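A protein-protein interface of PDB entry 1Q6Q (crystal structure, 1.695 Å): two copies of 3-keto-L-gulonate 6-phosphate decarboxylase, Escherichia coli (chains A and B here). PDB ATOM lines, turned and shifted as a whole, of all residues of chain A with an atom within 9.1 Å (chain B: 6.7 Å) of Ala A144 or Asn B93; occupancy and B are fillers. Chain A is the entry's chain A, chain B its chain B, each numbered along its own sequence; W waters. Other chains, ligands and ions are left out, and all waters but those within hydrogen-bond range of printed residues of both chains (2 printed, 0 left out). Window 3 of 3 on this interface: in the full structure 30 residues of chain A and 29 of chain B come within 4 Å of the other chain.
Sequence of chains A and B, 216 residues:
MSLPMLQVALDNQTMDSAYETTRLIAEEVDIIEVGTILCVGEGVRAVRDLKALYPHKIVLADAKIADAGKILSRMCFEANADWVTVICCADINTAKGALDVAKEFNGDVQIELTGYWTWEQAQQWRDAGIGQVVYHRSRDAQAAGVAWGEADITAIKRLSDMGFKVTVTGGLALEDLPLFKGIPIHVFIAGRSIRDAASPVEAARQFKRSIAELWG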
ATOM      1  N   ARG A 137     -20.635 -21.950  34.246  1.00  0.00           N
ATOM      2  CA  ARG A 137     -20.534 -20.522  34.046  1.00  0.00           C
ATOM      3  C   ARG A 137     -19.118 -20.178  33.639  1.00  0.00           C
ATOM      4  O   ARG A 137     -18.181 -20.500  34.338  1.00  0.00           O
ATOM      5  CB  ARG A 137     -21.007 -19.758  35.302  1.00  0.00           C
ATOM      6  CG  ARG A 137     -20.806 -18.217  35.229  1.00  0.00           C
ATOM      7  CD  ARG A 137     -21.377 -17.472  36.431  1.00  0.00           C
ATOM      8  NE  ARG A 137     -20.556 -17.696  37.618  1.00  0.00           N
ATOM      9  CZ  ARG A 137     -20.979 -17.566  38.879  1.00  0.00           C
ATOM     10  NH1 ARG A 137     -22.223 -17.138  39.165  1.00  0.00           N
ATOM     11  NH2 ARG A 137     -20.136 -17.820  39.867  1.00  0.00           N
ATOM     12  N   SER A 138     -18.957 -19.555  32.480  1.00  0.00           N
ATOM     13  CA  SER A 138     -17.651 -19.103  32.020  1.00  0.00           C
ATOM     14  C   SER A 138     -16.964 -18.068  32.935  1.00  0.00           C
ATOM     15  O   SER A 138     -17.561 -17.076  33.350  1.00  0.00           O
ATOM     16  CB  SER A 138     -17.736 -18.498  30.616  1.00  0.00           C
ATOM     17  OG  SER A 138     -16.539 -17.862  30.296  1.00  0.00           O
ATOM     18  N   ARG A 139     -15.677 -18.250  33.180  1.00  0.00           N
ATOM     19  CA  ARG A 139     -14.964 -17.278  33.976  1.00  0.00           C
ATOM     20  C   ARG A 139     -14.755 -15.996  33.222  1.00  0.00           C
ATOM     21  O   ARG A 139     -14.542 -14.974  33.823  1.00  0.00           O
ATOM     22  CB  ARG A 139     -13.644 -17.838  34.538  1.00  0.00           C
ATOM     23  CG  ARG A 139     -12.496 -17.776  33.604  1.00  0.00           C
ATOM     24  CD  ARG A 139     -11.196 -17.922  34.295  1.00  0.00           C
ATOM     25  NE  ARG A 139     -11.104 -19.205  34.936  1.00  0.00           N
ATOM     26  CZ  ARG A 139     -10.038 -19.628  35.610  1.00  0.00           C
ATOM     27  NH1 ARG A 139      -8.986 -18.836  35.765  1.00  0.00           N
ATOM     28  NH2 ARG A 139     -10.042 -20.854  36.144  1.00  0.00           N
ATOM     29  N   ASP A 140     -14.793 -16.055  31.890  1.00  0.00           N
ATOM     30  CA  ASP A 140     -14.579 -14.871  31.067  1.00  0.00           C
ATOM     31  C   ASP A 140     -15.830 -14.022  31.024  1.00  0.00           C
ATOM     32  O   ASP A 140     -15.749 -12.808  30.792  1.00  0.00           O
ATOM     33  CB  ASP A 140     -14.151 -15.288  29.671  1.00  0.00           C
ATOM     34  CG  ASP A 140     -12.774 -15.877  29.659  1.00  0.00           C
ATOM     35  OD1 ASP A 140     -11.980 -15.514  30.573  1.00  0.00           O
ATOM     36  OD2 ASP A 140     -12.396 -16.702  28.795  1.00  0.00           O
ATOM     37  N   ALA A 141     -16.972 -14.683  31.184  1.00  0.00           N
ATOM     38  CA  ALA A 141     -18.246 -14.007  31.367  1.00  0.00           C
ATOM     39  C   ALA A 141     -18.249 -13.431  32.791  1.00  0.00           C
ATOM     40  O   ALA A 141     -18.466 -12.247  32.948  1.00  0.00           O
ATOM     41  CB  ALA A 141     -19.389 -14.959  31.178  1.00  0.00           C
ATOM     42  N   GLN A 142     -17.908 -14.261  33.787  1.00  0.00           N
ATOM     43  CA  GLN A 142     -17.864 -13.845  35.208  1.00  0.00           C
ATOM     44  C   GLN A 142     -16.890 -12.694  35.474  1.00  0.00           C
ATOM     45  O   GLN A 142     -17.231 -11.756  36.191  1.00  0.00           O
ATOM     46  CB  GLN A 142     -17.510 -15.044  36.114  1.00  0.00           C
ATOM     47  N   ALA A 143     -15.666 -12.793  34.935  1.00  0.00           N
ATOM     48  CA  ALA A 143     -14.709 -11.671  34.891  1.00  0.00           C
ATOM     49  C   ALA A 143     -15.359 -10.365  34.366  1.00  0.00           C
ATOM     50  O   ALA A 143     -14.967  -9.259  34.767  1.00  0.00           O
ATOM     51  CB  ALA A 143     -13.486 -12.033  34.022  1.00  0.00           C
ATOM     52  N   ALA A 144     -16.322 -10.497  33.447  1.00  0.00           N
ATOM     53  CA  ALA A 144     -17.179  -9.373  33.045  1.00  0.00           C
ATOM     54  C   ALA A 144     -18.400  -9.335  33.948  1.00  0.00           C
ATOM     55  O   ALA A 144     -19.485  -9.700  33.522  1.00  0.00           O
ATOM     56  CB  ALA A 144     -17.606  -9.508  31.576  1.00  0.00           C
ATOM     57  N   VAL A 146     -21.028 -11.303  35.012  1.00  0.00           N
ATOM     58  CA  VAL A 146     -22.181 -12.209  35.068  1.00  0.00           C
ATOM     59  C   VAL A 146     -22.202 -12.934  36.424  1.00  0.00           C
ATOM     60  O   VAL A 146     -21.225 -13.602  36.773  1.00  0.00           O
ATOM     61  CB  VAL A 146     -22.133 -13.250  33.918  1.00  0.00           C
ATOM     62  CG1 VAL A 146     -23.363 -14.158  33.933  1.00  0.00           C
ATOM     63  CG2 VAL A 146     -21.987 -12.564  32.557  1.00  0.00           C
ATOM     64  N   ALA A 147     -23.311 -12.795  37.169  1.00  0.00           N
ATOM     65  CA  ALA A 147     -23.519 -13.436  38.487  1.00  0.00           C
ATOM     66  C   ALA A 147     -24.456 -14.680  38.369  1.00  0.00           C
ATOM     67  O   ALA A 147     -24.838 -15.026  37.239  1.00  0.00           O
ATOM     68  CB  ALA A 147     -24.089 -12.418  39.464  1.00  0.00           C
ATOM     69  N   GLY B  69      -9.726 -17.759  28.279  1.00  0.00           N
ATOM     70  CA  GLY B  69      -9.091 -17.354  27.031  1.00  0.00           C
ATOM     71  C   GLY B  69      -7.742 -16.723  27.227  1.00  0.00           C
ATOM     72  O   GLY B  69      -6.772 -17.041  26.493  1.00  0.00           O
ATOM     73  N   LYS B  70      -7.585 -15.889  28.264  1.00  0.00           N
ATOM     74  CA  LYS B  70      -6.284 -15.266  28.497  1.00  0.00           C
ATOM     75  C   LYS B  70      -5.214 -16.266  28.940  1.00  0.00           C
ATOM     76  O   LYS B  70      -4.089 -16.241  28.442  1.00  0.00           O
ATOM     77  CB  LYS B  70      -6.398 -14.122  29.537  1.00  0.00           C
ATOM     78  CG  LYS B  70      -5.084 -13.489  29.918  1.00  0.00           C
ATOM     79  CD  LYS B  70      -5.161 -12.390  31.009  1.00  0.00           C
ATOM     80  CE  LYS B  70      -5.820 -12.840  32.362  1.00  0.00           C
ATOM     81  NZ  LYS B  70      -5.805 -11.661  33.357  1.00  0.00           N
ATOM     82  N   ALA B  90     -17.532 -20.481  22.577  1.00  0.00           N
ATOM     83  CA  ALA B  90     -16.918 -19.753  23.707  1.00  0.00           C
ATOM     84  C   ALA B  90     -17.582 -18.392  23.868  1.00  0.00           C
ATOM     85  O   ALA B  90     -17.987 -17.742  22.905  1.00  0.00           O
ATOM     86  CB  ALA B  90     -15.423 -19.559  23.476  1.00  0.00           C
ATOM     87  N   ASP B  91     -17.629 -17.909  25.103  1.00  0.00           N
ATOM     88  CA  ASP B  91     -17.989 -16.503  25.351  1.00  0.00           C
ATOM     89  C   ASP B  91     -17.199 -15.529  24.492  1.00  0.00           C
ATOM     90  O   ASP B  91     -15.989 -15.690  24.268  1.00  0.00           O
ATOM     91  CB  ASP B  91     -17.786 -16.214  26.861  1.00  0.00           C
ATOM     92  CG  ASP B  91     -18.556 -15.002  27.320  1.00  0.00           C
ATOM     93  OD1 ASP B  91     -19.732 -15.156  27.652  1.00  0.00           O
ATOM     94  OD2 ASP B  91     -18.105 -13.859  27.239  1.00  0.00           O
ATOM     95  N   ILE B  92     -17.824 -14.481  23.976  1.00  0.00           N
ATOM     96  CA  ILE B  92     -17.113 -13.493  23.199  1.00  0.00           C
ATOM     97  C   ILE B  92     -15.922 -12.918  23.962  1.00  0.00           C
ATOM     98  O   ILE B  92     -14.909 -12.552  23.373  1.00  0.00           O
ATOM     99  CB  ILE B  92     -18.091 -12.382  22.733  1.00  0.00           C
ATOM    100  CG1 ILE B  92     -17.376 -11.365  21.868  1.00  0.00           C
ATOM    101  CG2 ILE B  92     -18.664 -11.639  23.978  1.00  0.00           C
ATOM    102  CD1 ILE B  92     -16.748 -11.893  20.533  1.00  0.00           C
ATOM    103  N   ASN B  93     -15.987 -12.894  25.306  1.00  0.00           N
ATOM    104  CA  ASN B  93     -14.849 -12.378  26.057  1.00  0.00           C
ATOM    105  C   ASN B  93     -13.682 -13.355  26.123  1.00  0.00           C
ATOM    106  O   ASN B  93     -12.537 -12.921  26.339  1.00  0.00           O
ATOM    107  CB  ASN B  93     -15.247 -11.956  27.476  1.00  0.00           C
ATOM    108  CG  ASN B  93     -16.148 -10.728  27.459  1.00  0.00           C
ATOM    109  OD1 ASN B  93     -15.793  -9.689  26.868  1.00  0.00           O
ATOM    110  ND2 ASN B  93     -17.334 -10.882  27.980  1.00  0.00           N
ATOM    111  N   THR B  94     -13.996 -14.632  25.947  1.00  0.00           N
ATOM    112  CA  THR B  94     -12.949 -15.648  25.755  1.00  0.00           C
ATOM    113  C   THR B  94     -12.182 -15.348  24.484  1.00  0.00           C
ATOM    114  O   THR B  94     -10.977 -15.304  24.502  1.00  0.00           O
ATOM    115  CB  THR B  94     -13.549 -17.078  25.741  1.00  0.00           C
ATOM    116  OG1 THR B  94     -14.191 -17.349  26.986  1.00  0.00           O
ATOM    117  CG2 THR B  94     -12.419 -18.148  25.554  1.00  0.00           C
ATOM    118  N   ALA B  95     -12.870 -15.078  23.370  1.00  0.00           N
ATOM    119  CA  ALA B  95     -12.169 -14.726  22.146  1.00  0.00           C
ATOM    120  C   ALA B  95     -11.399 -13.410  22.285  1.00  0.00           C
ATOM    121  O   ALA B  95     -10.234 -13.279  21.899  1.00  0.00           O
ATOM    122  CB  ALA B  95     -13.176 -14.675  20.992  1.00  0.00           C
ATOM    123  N   LYS B  96     -12.035 -12.390  22.872  1.00  0.00           N
ATOM    124  CA  LYS B  96     -11.359 -11.150  23.072  1.00  0.00           C
ATOM    125  C   LYS B  96     -10.123 -11.263  23.912  1.00  0.00           C
ATOM    126  O   LYS B  96      -9.127 -10.646  23.634  1.00  0.00           O
ATOM    127  CB  LYS B  96     -12.307 -10.084  23.701  1.00  0.00           C
ATOM    128  CG  LYS B  96     -13.403  -9.616  22.790  1.00  0.00           C
ATOM    129  CD  LYS B  96     -14.241  -8.518  23.512  1.00  0.00           C
ATOM    130  CE  LYS B  96     -15.233  -7.884  22.573  1.00  0.00           C
ATOM    131  NZ  LYS B  96     -15.715  -6.569  23.117  1.00  0.00           N
ATOM    132  N   GLY B  97     -10.188 -12.085  24.958  1.00  0.00           N
ATOM    133  CA  GLY B  97      -9.084 -12.222  25.871  1.00  0.00           C
ATOM    134  C   GLY B  97      -7.940 -12.911  25.184  1.00  0.00           C
ATOM    135  O   GLY B  97      -6.789 -12.526  25.373  1.00  0.00           O
ATOM    136  N   ALA B  98      -8.273 -13.944  24.399  1.00  0.00           N
ATOM    137  CA  ALA B  98      -7.251 -14.642  23.615  1.00  0.00           C
ATOM    138  C   ALA B  98      -6.606 -13.683  22.579  1.00  0.00           C
ATOM    139  O   ALA B  98      -5.425 -13.725  22.374  1.00  0.00           O
ATOM    140  CB  ALA B  98      -7.877 -15.878  22.915  1.00  0.00           C
HETATM  141  O   HOH W   1     -16.251 -19.228  27.481  1.00  0.00           O
HETATM  142  O   HOH W   2      -9.582 -14.729  29.807  1.00  0.00           O
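The backbone NH (N) of Gly B69 sits at hydrogen-bond distance from the side-chain carboxylate (OD2) of Asp A140 (2.9 Å). The side-chain carboxylate (OD2) of Asp A140 lies within hydrogen-bond range of the side-chain hydroxyl (OG1) of Thr B94, 2.6 Å away.
N of Asp A140 sits at hydrogen-bond distance from OG of Ser A138 (3.0 Å). The backbone NH (N) of Ala A141 is in hydrogen-bond range of the side-chain hydroxyl (OG) of Ser A138, 3.3 Å away. O of Ala A141 lies within hydrogen-bond range of N of Val A146, 3.4 Å away. The side-chain carboxylate of Asp B91 sits close to the backbone NH of Asn B93 (3.0 Å).
Water W2 lies within hydrogen-bond range of the side-chain carboxylate (OD1) of Asp A140, the backbone NH (N) of Lys B70 and the backbone NH (N) of Gly B69. Water W1 lies within hydrogen-bond range of the side-chain hydroxyl (OG1) of Thr B94 (2.8 Å), the backbone NH (N) of Asp B91 (3.0 Å) and the side-chain hydroxyl (OG) of Ser A138 (3.1 Å).
Of the 10 printed residues of chain A, 3 touch a printed residue of chain B. Among the printed residues, no Asp or Glu carboxylate lies within 4 Å of a Lys or Arg side-chain nitrogen of the other chain.
Of the printed residues of chain B, Ala A144 touches Asn B93 (3.9 Å). No residue of chain A comes within 4 Å of Ile B92. Thr B94 touches just one residue of chain A: Asp A140 (2.6 Å). Lys B96 touches none of the printed residues of chain A. Of the printed residues of chain A, Gly B69 touches Asp A140 (2.9 Å). Of the printed residues of chain B, Ala A141 touches Asp B91. Ser A138 touches none of the printed residues of chain B. Ala A147 touches none of the printed residues of chain B. The nearest residue of chain A that does not touch Asn B93 is Ala A141 (4.7 Å).
No position is printed for both chains.
Asn B93 touches Asp A140. CB of Ala A141 touches OD1 of Asp B91 (3.5 Å). Ala A144 touches Asn B93.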
